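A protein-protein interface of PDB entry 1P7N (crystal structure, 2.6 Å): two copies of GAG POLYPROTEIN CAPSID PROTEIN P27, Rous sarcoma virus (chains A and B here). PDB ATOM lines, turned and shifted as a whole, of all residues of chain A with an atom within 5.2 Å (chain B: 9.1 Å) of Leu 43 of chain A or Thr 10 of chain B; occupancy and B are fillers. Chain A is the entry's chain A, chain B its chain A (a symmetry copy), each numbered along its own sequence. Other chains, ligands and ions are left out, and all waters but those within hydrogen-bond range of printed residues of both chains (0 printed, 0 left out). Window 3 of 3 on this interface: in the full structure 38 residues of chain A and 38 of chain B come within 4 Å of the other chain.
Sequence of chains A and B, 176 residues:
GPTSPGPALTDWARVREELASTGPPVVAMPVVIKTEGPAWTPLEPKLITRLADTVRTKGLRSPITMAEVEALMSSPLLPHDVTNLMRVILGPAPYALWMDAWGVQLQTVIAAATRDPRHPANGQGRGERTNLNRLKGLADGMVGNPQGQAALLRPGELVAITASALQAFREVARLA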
ATOM      1  N   THR A  41      -6.471  11.029 -22.039  1.00  0.00           N
ATOM      2  CA  THR A  41      -7.233  10.375 -20.989  1.00  0.00           C
ATOM      3  C   THR A  41      -6.317  10.010 -19.826  1.00  0.00           C
ATOM      4  O   THR A  41      -5.221   9.519 -20.033  1.00  0.00           O
ATOM      5  CB  THR A  41      -7.889   9.068 -21.497  1.00  0.00           C
ATOM      6  OG1 THR A  41      -8.654   9.341 -22.675  1.00  0.00           O
ATOM      7  CG2 THR A  41      -8.818   8.493 -20.445  1.00  0.00           C
ATOM      8  N   PRO A  42      -6.746  10.274 -18.588  1.00  0.00           N
ATOM      9  CA  PRO A  42      -5.893   9.921 -17.453  1.00  0.00           C
ATOM     10  C   PRO A  42      -6.151   8.476 -17.073  1.00  0.00           C
ATOM     11  O   PRO A  42      -7.273   7.987 -17.217  1.00  0.00           O
ATOM     12  CB  PRO A  42      -6.348  10.888 -16.367  1.00  0.00           C
ATOM     13  CG  PRO A  42      -7.794  11.040 -16.664  1.00  0.00           C
ATOM     14  CD  PRO A  42      -7.822  11.185 -18.166  1.00  0.00           C
ATOM     15  N   LEU A  43      -5.119   7.794 -16.591  1.00  0.00           N
ATOM     16  CA  LEU A  43      -5.248   6.404 -16.191  1.00  0.00           C
ATOM     17  C   LEU A  43      -5.635   6.298 -14.718  1.00  0.00           C
ATOM     18  O   LEU A  43      -5.244   7.125 -13.907  1.00  0.00           O
ATOM     19  CB  LEU A  43      -3.930   5.686 -16.435  1.00  0.00           C
ATOM     20  CG  LEU A  43      -3.388   5.687 -17.864  1.00  0.00           C
ATOM     21  CD1 LEU A  43      -1.929   5.262 -17.832  1.00  0.00           C
ATOM     22  CD2 LEU A  43      -4.191   4.761 -18.733  1.00  0.00           C
ATOM     23  N   GLU A  44      -6.410   5.275 -14.375  1.00  0.00           N
ATOM     24  CA  GLU A  44      -6.858   5.065 -12.997  1.00  0.00           C
ATOM     25  C   GLU A  44      -5.862   4.167 -12.279  1.00  0.00           C
ATOM     26  O   GLU A  44      -5.584   3.052 -12.715  1.00  0.00           O
ATOM     27  CB  GLU A  44      -8.245   4.420 -12.994  1.00  0.00           C
ATOM     28  CG  GLU A  44      -9.000   4.542 -11.671  1.00  0.00           C
ATOM     29  CD  GLU A  44      -8.355   3.753 -10.544  1.00  0.00           C
ATOM     30  OE1 GLU A  44      -7.951   2.593 -10.784  1.00  0.00           O
ATOM     31  OE2 GLU A  44      -8.265   4.289  -9.423  1.00  0.00           O
ATOM     32  N   PRO A  45      -5.306   4.646 -11.158  1.00  0.00           N
ATOM     33  CA  PRO A  45      -4.333   3.861 -10.396  1.00  0.00           C
ATOM     34  C   PRO A  45      -4.646   2.369 -10.266  1.00  0.00           C
ATOM     35  O   PRO A  45      -3.808   1.536 -10.605  1.00  0.00           O
ATOM     36  CB  PRO A  45      -4.302   4.579  -9.049  1.00  0.00           C
ATOM     37  CG  PRO A  45      -4.493   6.006  -9.440  1.00  0.00           C
ATOM     38  CD  PRO A  45      -5.590   5.931 -10.487  1.00  0.00           C
ATOM     39  N   ILE A  48      -4.070   0.428 -13.186  1.00  0.00           N
ATOM     40  CA  ILE A  48      -2.639   0.311 -13.479  1.00  0.00           C
ATOM     41  C   ILE A  48      -1.976  -0.785 -12.653  1.00  0.00           C
ATOM     42  O   ILE A  48      -1.122  -1.521 -13.150  1.00  0.00           O
ATOM     43  CB  ILE A  48      -1.893   1.636 -13.234  1.00  0.00           C
ATOM     44  CG1 ILE A  48      -2.247   2.640 -14.339  1.00  0.00           C
ATOM     45  CG2 ILE A  48      -0.403   1.395 -13.224  1.00  0.00           C
ATOM     46  CD1 ILE A  48      -1.702   4.027 -14.121  1.00  0.00           C
ATOM     47  N   LEU A  72      -5.993  -0.759 -22.647  1.00  0.00           N
ATOM     48  CA  LEU A  72      -5.638   0.403 -21.852  1.00  0.00           C
ATOM     49  C   LEU A  72      -4.980   1.514 -22.664  1.00  0.00           C
ATOM     50  O   LEU A  72      -4.891   2.652 -22.216  1.00  0.00           O
ATOM     51  CB  LEU A  72      -4.703  -0.023 -20.723  1.00  0.00           C
ATOM     52  CG  LEU A  72      -4.397   1.044 -19.678  1.00  0.00           C
ATOM     53  CD1 LEU A  72      -5.715   1.585 -19.136  1.00  0.00           C
ATOM     54  CD2 LEU A  72      -3.549   0.463 -18.556  1.00  0.00           C
ATOM     55  N   LEU A  77      -2.939   9.260 -24.754  1.00  0.00           N
ATOM     56  CA  LEU A  77      -2.249   9.480 -23.504  1.00  0.00           C
ATOM     57  C   LEU A  77      -1.145  10.509 -23.702  1.00  0.00           C
ATOM     58  O   LEU A  77      -0.670  10.715 -24.822  1.00  0.00           O
ATOM     59  CB  LEU A  77      -1.650   8.160 -23.006  1.00  0.00           C
ATOM     60  CG  LEU A  77      -2.650   7.072 -22.594  1.00  0.00           C
ATOM     61  CD1 LEU A  77      -1.925   5.806 -22.178  1.00  0.00           C
ATOM     62  CD2 LEU A  77      -3.472   7.565 -21.441  1.00  0.00           C
ATOM     63  N   ASP A  81       2.455   9.957 -19.325  1.00  0.00           N
ATOM     64  CA  ASP A  81       1.689   8.789 -18.974  1.00  0.00           C
ATOM     65  C   ASP A  81       2.188   7.520 -19.624  1.00  0.00           C
ATOM     66  O   ASP A  81       2.354   6.510 -18.944  1.00  0.00           O
ATOM     67  CB  ASP A  81       0.227   9.010 -19.331  1.00  0.00           C
ATOM     68  CG  ASP A  81      -0.494   9.897 -18.329  1.00  0.00           C
ATOM     69  OD1 ASP A  81       0.100  10.235 -17.271  1.00  0.00           O
ATOM     70  OD2 ASP A  81      -1.670  10.241 -18.614  1.00  0.00           O
ATOM     71  N   LEU A  85       3.678   4.552 -17.547  1.00  0.00           N
ATOM     72  CA  LEU A  85       2.986   3.285 -17.653  1.00  0.00           C
ATOM     73  C   LEU A  85       3.990   2.199 -17.984  1.00  0.00           C
ATOM     74  O   LEU A  85       4.052   1.171 -17.331  1.00  0.00           O
ATOM     75  CB  LEU A  85       1.928   3.345 -18.744  1.00  0.00           C
ATOM     76  CG  LEU A  85       1.255   1.992 -18.973  1.00  0.00           C
ATOM     77  CD1 LEU A  85       0.468   1.621 -17.735  1.00  0.00           C
ATOM     78  CD2 LEU A  85       0.369   2.049 -20.203  1.00  0.00           C
ATOM     79  N   THR B   3      -8.223  14.083  -5.570  1.00  0.00           N
ATOM     80  CA  THR B   3      -7.815  12.894  -6.307  1.00  0.00           C
ATOM     81  C   THR B   3      -8.753  11.723  -6.029  1.00  0.00           C
ATOM     82  O   THR B   3      -8.661  10.679  -6.675  1.00  0.00           O
ATOM     83  CB  THR B   3      -6.380  12.473  -5.936  1.00  0.00           C
ATOM     84  OG1 THR B   3      -6.298  12.229  -4.526  1.00  0.00           O
ATOM     85  CG2 THR B   3      -5.391  13.564  -6.316  1.00  0.00           C
ATOM     86  N   GLY B   6     -12.048  12.183  -9.104  1.00  0.00           N
ATOM     87  CA  GLY B   6     -11.432  11.858 -10.379  1.00  0.00           C
ATOM     88  C   GLY B   6     -10.125  12.606 -10.586  1.00  0.00           C
ATOM     89  O   GLY B   6     -10.071  13.815 -10.332  1.00  0.00           O
ATOM     90  N   PRO B   7      -9.049  11.917 -11.030  1.00  0.00           N
ATOM     91  CA  PRO B   7      -7.720  12.511 -11.277  1.00  0.00           C
ATOM     92  C   PRO B   7      -7.545  13.124 -12.683  1.00  0.00           C
ATOM     93  O   PRO B   7      -7.278  12.392 -13.643  1.00  0.00           O
ATOM     94  CB  PRO B   7      -6.754  11.330 -11.063  1.00  0.00           C
ATOM     95  CG  PRO B   7      -7.593  10.263 -10.348  1.00  0.00           C
ATOM     96  CD  PRO B   7      -8.949  10.447 -10.975  1.00  0.00           C
ATOM     97  N   ALA B   8      -7.686  14.448 -12.806  1.00  0.00           N
ATOM     98  CA  ALA B   8      -7.526  15.104 -14.103  1.00  0.00           C
ATOM     99  C   ALA B   8      -6.231  14.581 -14.699  1.00  0.00           C
ATOM    100  O   ALA B   8      -6.200  14.071 -15.816  1.00  0.00           O
ATOM    101  CB  ALA B   8      -7.450  16.606 -13.935  1.00  0.00           C
ATOM    102  N   LEU B   9      -5.159  14.702 -13.932  1.00  0.00           N
ATOM    103  CA  LEU B   9      -3.858  14.223 -14.361  1.00  0.00           C
ATOM    104  C   LEU B   9      -3.635  12.919 -13.620  1.00  0.00           C
ATOM    105  O   LEU B   9      -3.854  12.842 -12.418  1.00  0.00           O
ATOM    106  CB  LEU B   9      -2.780  15.240 -13.989  1.00  0.00           C
ATOM    107  CG  LEU B   9      -2.044  15.993 -15.107  1.00  0.00           C
ATOM    108  CD1 LEU B   9      -2.970  16.400 -16.236  1.00  0.00           C
ATOM    109  CD2 LEU B   9      -1.376  17.215 -14.481  1.00  0.00           C
ATOM    110  N   THR B  10      -3.221  11.886 -14.339  1.00  0.00           N
ATOM    111  CA  THR B  10      -2.974  10.599 -13.717  1.00  0.00           C
ATOM    112  C   THR B  10      -2.231  10.807 -12.414  1.00  0.00           C
ATOM    113  O   THR B  10      -1.155  11.409 -12.393  1.00  0.00           O
ATOM    114  CB  THR B  10      -2.124   9.710 -14.607  1.00  0.00           C
ATOM    115  OG1 THR B  10      -2.722   9.627 -15.906  1.00  0.00           O
ATOM    116  CG2 THR B  10      -2.018   8.333 -14.013  1.00  0.00           C
ATOM    117  N   ASP B  11      -2.814  10.318 -11.322  1.00  0.00           N
ATOM    118  CA  ASP B  11      -2.203  10.452 -10.007  1.00  0.00           C
ATOM    119  C   ASP B  11      -1.171   9.356  -9.875  1.00  0.00           C
ATOM    120  O   ASP B  11      -1.488   8.239  -9.444  1.00  0.00           O
ATOM    121  CB  ASP B  11      -3.256  10.294  -8.915  1.00  0.00           C
ATOM    122  CG  ASP B  11      -2.669  10.370  -7.524  1.00  0.00           C
ATOM    123  OD1 ASP B  11      -3.175   9.651  -6.646  1.00  0.00           O
ATOM    124  OD2 ASP B  11      -1.719  11.145  -7.302  1.00  0.00           O
ATOM    125  N   TRP B  12       0.066   9.666 -10.245  1.00  0.00           N
ATOM    126  CA  TRP B  12       1.107   8.664 -10.165  1.00  0.00           C
ATOM    127  C   TRP B  12       1.651   8.469  -8.755  1.00  0.00           C
ATOM    128  O   TRP B  12       2.370   7.499  -8.488  1.00  0.00           O
ATOM    129  CB  TRP B  12       2.226   8.999 -11.139  1.00  0.00           C
ATOM    130  CG  TRP B  12       1.868   8.727 -12.580  1.00  0.00           C
ATOM    131  CD1 TRP B  12       1.599   9.651 -13.547  1.00  0.00           C
ATOM    132  CD2 TRP B  12       1.783   7.442 -13.217  1.00  0.00           C
ATOM    133  NE1 TRP B  12       1.361   9.025 -14.744  1.00  0.00           N
ATOM    134  CE2 TRP B  12       1.469   7.669 -14.571  1.00  0.00           C
ATOM    135  CE3 TRP B  12       1.947   6.128 -12.774  1.00  0.00           C
ATOM    136  CZ2 TRP B  12       1.322   6.632 -15.492  1.00  0.00           C
ATOM    137  CZ3 TRP B  12       1.803   5.085 -13.700  1.00  0.00           C
ATOM    138  CH2 TRP B  12       1.495   5.350 -15.041  1.00  0.00           C
ATOM    139  N   ALA B  13       1.301   9.377  -7.848  1.00  0.00           N
ATOM    140  CA  ALA B  13       1.739   9.260  -6.466  1.00  0.00           C
ATOM    141  C   ALA B  13       1.102   7.992  -5.911  1.00  0.00           C
ATOM    142  O   ALA B  13       1.775   7.169  -5.292  1.00  0.00           O
ATOM    143  CB  ALA B  13       1.294  10.463  -5.669  1.00  0.00           C
ATOM    144  N   ARG B  14      -0.197   7.835  -6.154  1.00  0.00           N
ATOM    145  CA  ARG B  14      -0.932   6.660  -5.696  1.00  0.00           C
ATOM    146  C   ARG B  14      -0.347   5.388  -6.285  1.00  0.00           C
ATOM    147  O   ARG B  14      -0.107   4.420  -5.569  1.00  0.00           O
ATOM    148  CB  ARG B  14      -2.411   6.773  -6.075  1.00  0.00           C
ATOM    149  CG  ARG B  14      -3.339   7.160  -4.919  1.00  0.00           C
ATOM    150  CD  ARG B  14      -2.847   8.409  -4.169  1.00  0.00           C
ATOM    151  NE  ARG B  14      -3.745   8.784  -3.077  1.00  0.00           N
ATOM    152  CZ  ARG B  14      -4.989   9.232  -3.240  1.00  0.00           C
ATOM    153  NH1 ARG B  14      -5.501   9.373  -4.459  1.00  0.00           N
ATOM    154  NH2 ARG B  14      -5.729   9.532  -2.178  1.00  0.00           N
ATOM    155  N   VAL B  15      -0.116   5.384  -7.593  1.00  0.00           N
ATOM    156  CA  VAL B  15       0.453   4.215  -8.245  1.00  0.00           C
ATOM    157  C   VAL B  15       1.754   3.863  -7.532  1.00  0.00           C
ATOM    158  O   VAL B  15       1.979   2.709  -7.185  1.00  0.00           O
ATOM    159  CB  VAL B  15       0.742   4.481  -9.744  1.00  0.00           C
ATOM    160  CG1 VAL B  15       1.238   3.221 -10.419  1.00  0.00           C
ATOM    161  CG2 VAL B  15      -0.510   4.987 -10.427  1.00  0.00           C
ATOM    162  N   ARG B  16       2.609   4.856  -7.302  1.00  0.00           N
ATOM    163  CA  ARG B  16       3.867   4.598  -6.609  1.00  0.00           C
ATOM    164  C   ARG B  16       3.565   3.800  -5.345  1.00  0.00           C
ATOM    165  O   ARG B  16       3.956   2.641  -5.219  1.00  0.00           O
ATOM    166  CB  ARG B  16       4.575   5.919  -6.253  1.00  0.00           C
ATOM    167  CG  ARG B  16       5.840   5.762  -5.410  1.00  0.00           C
ATOM    168  CD  ARG B  16       6.559   7.093  -5.157  1.00  0.00           C
ATOM    169  NE  ARG B  16       7.520   7.394  -6.219  1.00  0.00           N
ATOM    170  CZ  ARG B  16       8.719   6.819  -6.350  1.00  0.00           C
ATOM    171  NH1 ARG B  16       9.133   5.906  -5.470  1.00  0.00           N
ATOM    172  NH2 ARG B  16       9.492   7.127  -7.390  1.00  0.00           N
ATOM    173  N   PRO B  30       7.505   4.719 -10.756  1.00  0.00           N
ATOM    174  CA  PRO B  30       7.080   5.570 -11.872  1.00  0.00           C
ATOM    175  C   PRO B  30       7.537   6.984 -11.461  1.00  0.00           C
ATOM    176  O   PRO B  30       7.563   7.300 -10.275  1.00  0.00           O
ATOM    177  CB  PRO B  30       5.560   5.413 -11.864  1.00  0.00           C
ATOM    178  CG  PRO B  30       5.268   5.293 -10.421  1.00  0.00           C
ATOM    179  CD  PRO B  30       6.347   4.361  -9.912  1.00  0.00           C
ATOM    180  N   VAL B  31       7.922   7.818 -12.416  1.00  0.00           N
ATOM    181  CA  VAL B  31       8.372   9.168 -12.089  1.00  0.00           C
ATOM    182  C   VAL B  31       7.216   9.983 -11.548  1.00  0.00           C
ATOM    183  O   VAL B  31       6.321  10.350 -12.297  1.00  0.00           O
ATOM    184  CB  VAL B  31       8.936   9.886 -13.328  1.00  0.00           C
ATOM    185  CG1 VAL B  31       9.377  11.280 -12.961  1.00  0.00           C
ATOM    186  CG2 VAL B  31      10.088   9.098 -13.903  1.00  0.00           C
ATOM    187  N   VAL B  32       7.245  10.270 -10.250  1.00  0.00           N
ATOM    188  CA  VAL B  32       6.185  11.038  -9.593  1.00  0.00           C
ATOM    189  C   VAL B  32       6.565  12.499  -9.398  1.00  0.00           C
ATOM    190  O   VAL B  32       7.234  12.876  -8.433  1.00  0.00           O
ATOM    191  CB  VAL B  32       5.829  10.427  -8.225  1.00  0.00           C
ATOM    192  CG1 VAL B  32       4.821  11.292  -7.512  1.00  0.00           C
ATOM    193  CG2 VAL B  32       5.278   9.029  -8.420  1.00  0.00           C
ATOM    194  N   ILE B  33       6.110  13.324 -10.326  1.00  0.00           N
ATOM    195  CA  ILE B  33       6.382  14.748 -10.309  1.00  0.00           C
ATOM    196  C   ILE B  33       5.564  15.562  -9.287  1.00  0.00           C
ATOM    197  O   ILE B  33       6.129  16.177  -8.368  1.00  0.00           O
ATOM    198  CB  ILE B  33       6.192  15.299 -11.729  1.00  0.00           C
ATOM    199  CG1 ILE B  33       7.408  14.895 -12.574  1.00  0.00           C
ATOM    200  CG2 ILE B  33       5.958  16.797 -11.698  1.00  0.00           C
ATOM    201  CD1 ILE B  33       7.180  14.904 -14.075  1.00  0.00           C
ATOM    202  N   LYS B  34       4.246  15.570  -9.433  1.00  0.00           N
ATOM    203  CA  LYS B  34       3.406  16.326  -8.510  1.00  0.00           C
ATOM    204  C   LYS B  34       3.527  17.849  -8.666  1.00  0.00           C
ATOM    205  O   LYS B  34       3.819  18.557  -7.700  1.00  0.00           O
ATOM    206  CB  LYS B  34       3.714  15.961  -7.044  1.00  0.00           C
ATOM    207  CG  LYS B  34       3.245  14.571  -6.595  1.00  0.00           C
ATOM    208  CD  LYS B  34       3.328  14.407  -5.073  1.00  0.00           C
ATOM    209  CE  LYS B  34       4.733  14.697  -4.539  1.00  0.00           C
ATOM    210  NZ  LYS B  34       4.810  14.595  -3.052  1.00  0.00           N
ATOM    211  N   THR B  35       3.335  18.351  -9.883  1.00  0.00           N
ATOM    212  CA  THR B  35       3.360  19.797 -10.095  1.00  0.00           C
ATOM    213  C   THR B  35       1.973  20.152  -9.573  1.00  0.00           C
ATOM    214  O   THR B  35       0.975  19.615 -10.062  1.00  0.00           O
ATOM    215  CB  THR B  35       3.450  20.180 -11.602  1.00  0.00           C
ATOM    216  OG1 THR B  35       4.732  19.802 -12.126  1.00  0.00           O
ATOM    217  CG2 THR B  35       3.240  21.691 -11.783  1.00  0.00           C
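The backbone NH (N) of Leu 43 of chain A is in hydrogen-bond range of the side-chain hydroxyl (OG1) of Thr 10 of chain B (3.1 Å). OD2 of Asp 81 of chain A sits at hydrogen-bond distance from OG1 of Thr 10 of chain B. NE1 of Trp 12 of chain B is in hydrogen-bond range of OD1 of Asp 81 of chain A (3.1 Å).
The side-chain carboxylate (OD1) of Asp 11 of chain B lies within salt-bridge range of the guanidinium group (NH1) of Arg 14 of chain B, 3.2 Å away.
Among the printed residues, merely in contact across the chains: Pro 42 of chain A with Pro 7 of chain B, Pro 42 of chain A with Ala 8 of chain B, Pro 42 of chain A with Thr 10 of chain B, Pro 45 of chain A with Asp 11 of chain B, Pro 45 of chain A with Val 15 of chain B, Ile 48 of chain A with Trp 12 of chain B, Ile 48 of chain A with Val 15 of chain B and Leu 85 of chain A with Trp 12 of chain B.
Of chain B, only Thr 10 (3.1 Å) comes within 4 Å of Leu 43 of chain A. Of chain A, only Pro 42, Leu 43 and Asp 81 come within 4 Å of Thr 10 of chain B. Of the printed residues of chain B, Ile 48 of chain A touches Trp 12 (3.6 Å) and Val 15 (3.7 Å). Of the printed residues of chain A, Pro 7 of chain B touches Pro 42. Ile 33 of chain B touches none of the printed residues of chain A.
Printed residues of chain B that touch a printed residue of chain A: Pro 7, Ala 8, Thr 10, Asp 11, Trp 12 and Val 15. Along chain B the printed residues that touch a printed residue of chain A span positions 7 to 15. Of the 10 printed residues of chain A, 6 touch a printed residue of chain B. Hydrophobic or aromatic side chains of chain A that line the printed part of chain B: Pro 42, Pro 45 and Ile 48. Among the printed residues, 11 pairs touch across the chains. Among the printed residues, no Asp or Glu carboxylate lies within 4 Å of a Lys or Arg side-chain nitrogen of the other chain.
No position is printed for both chains.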
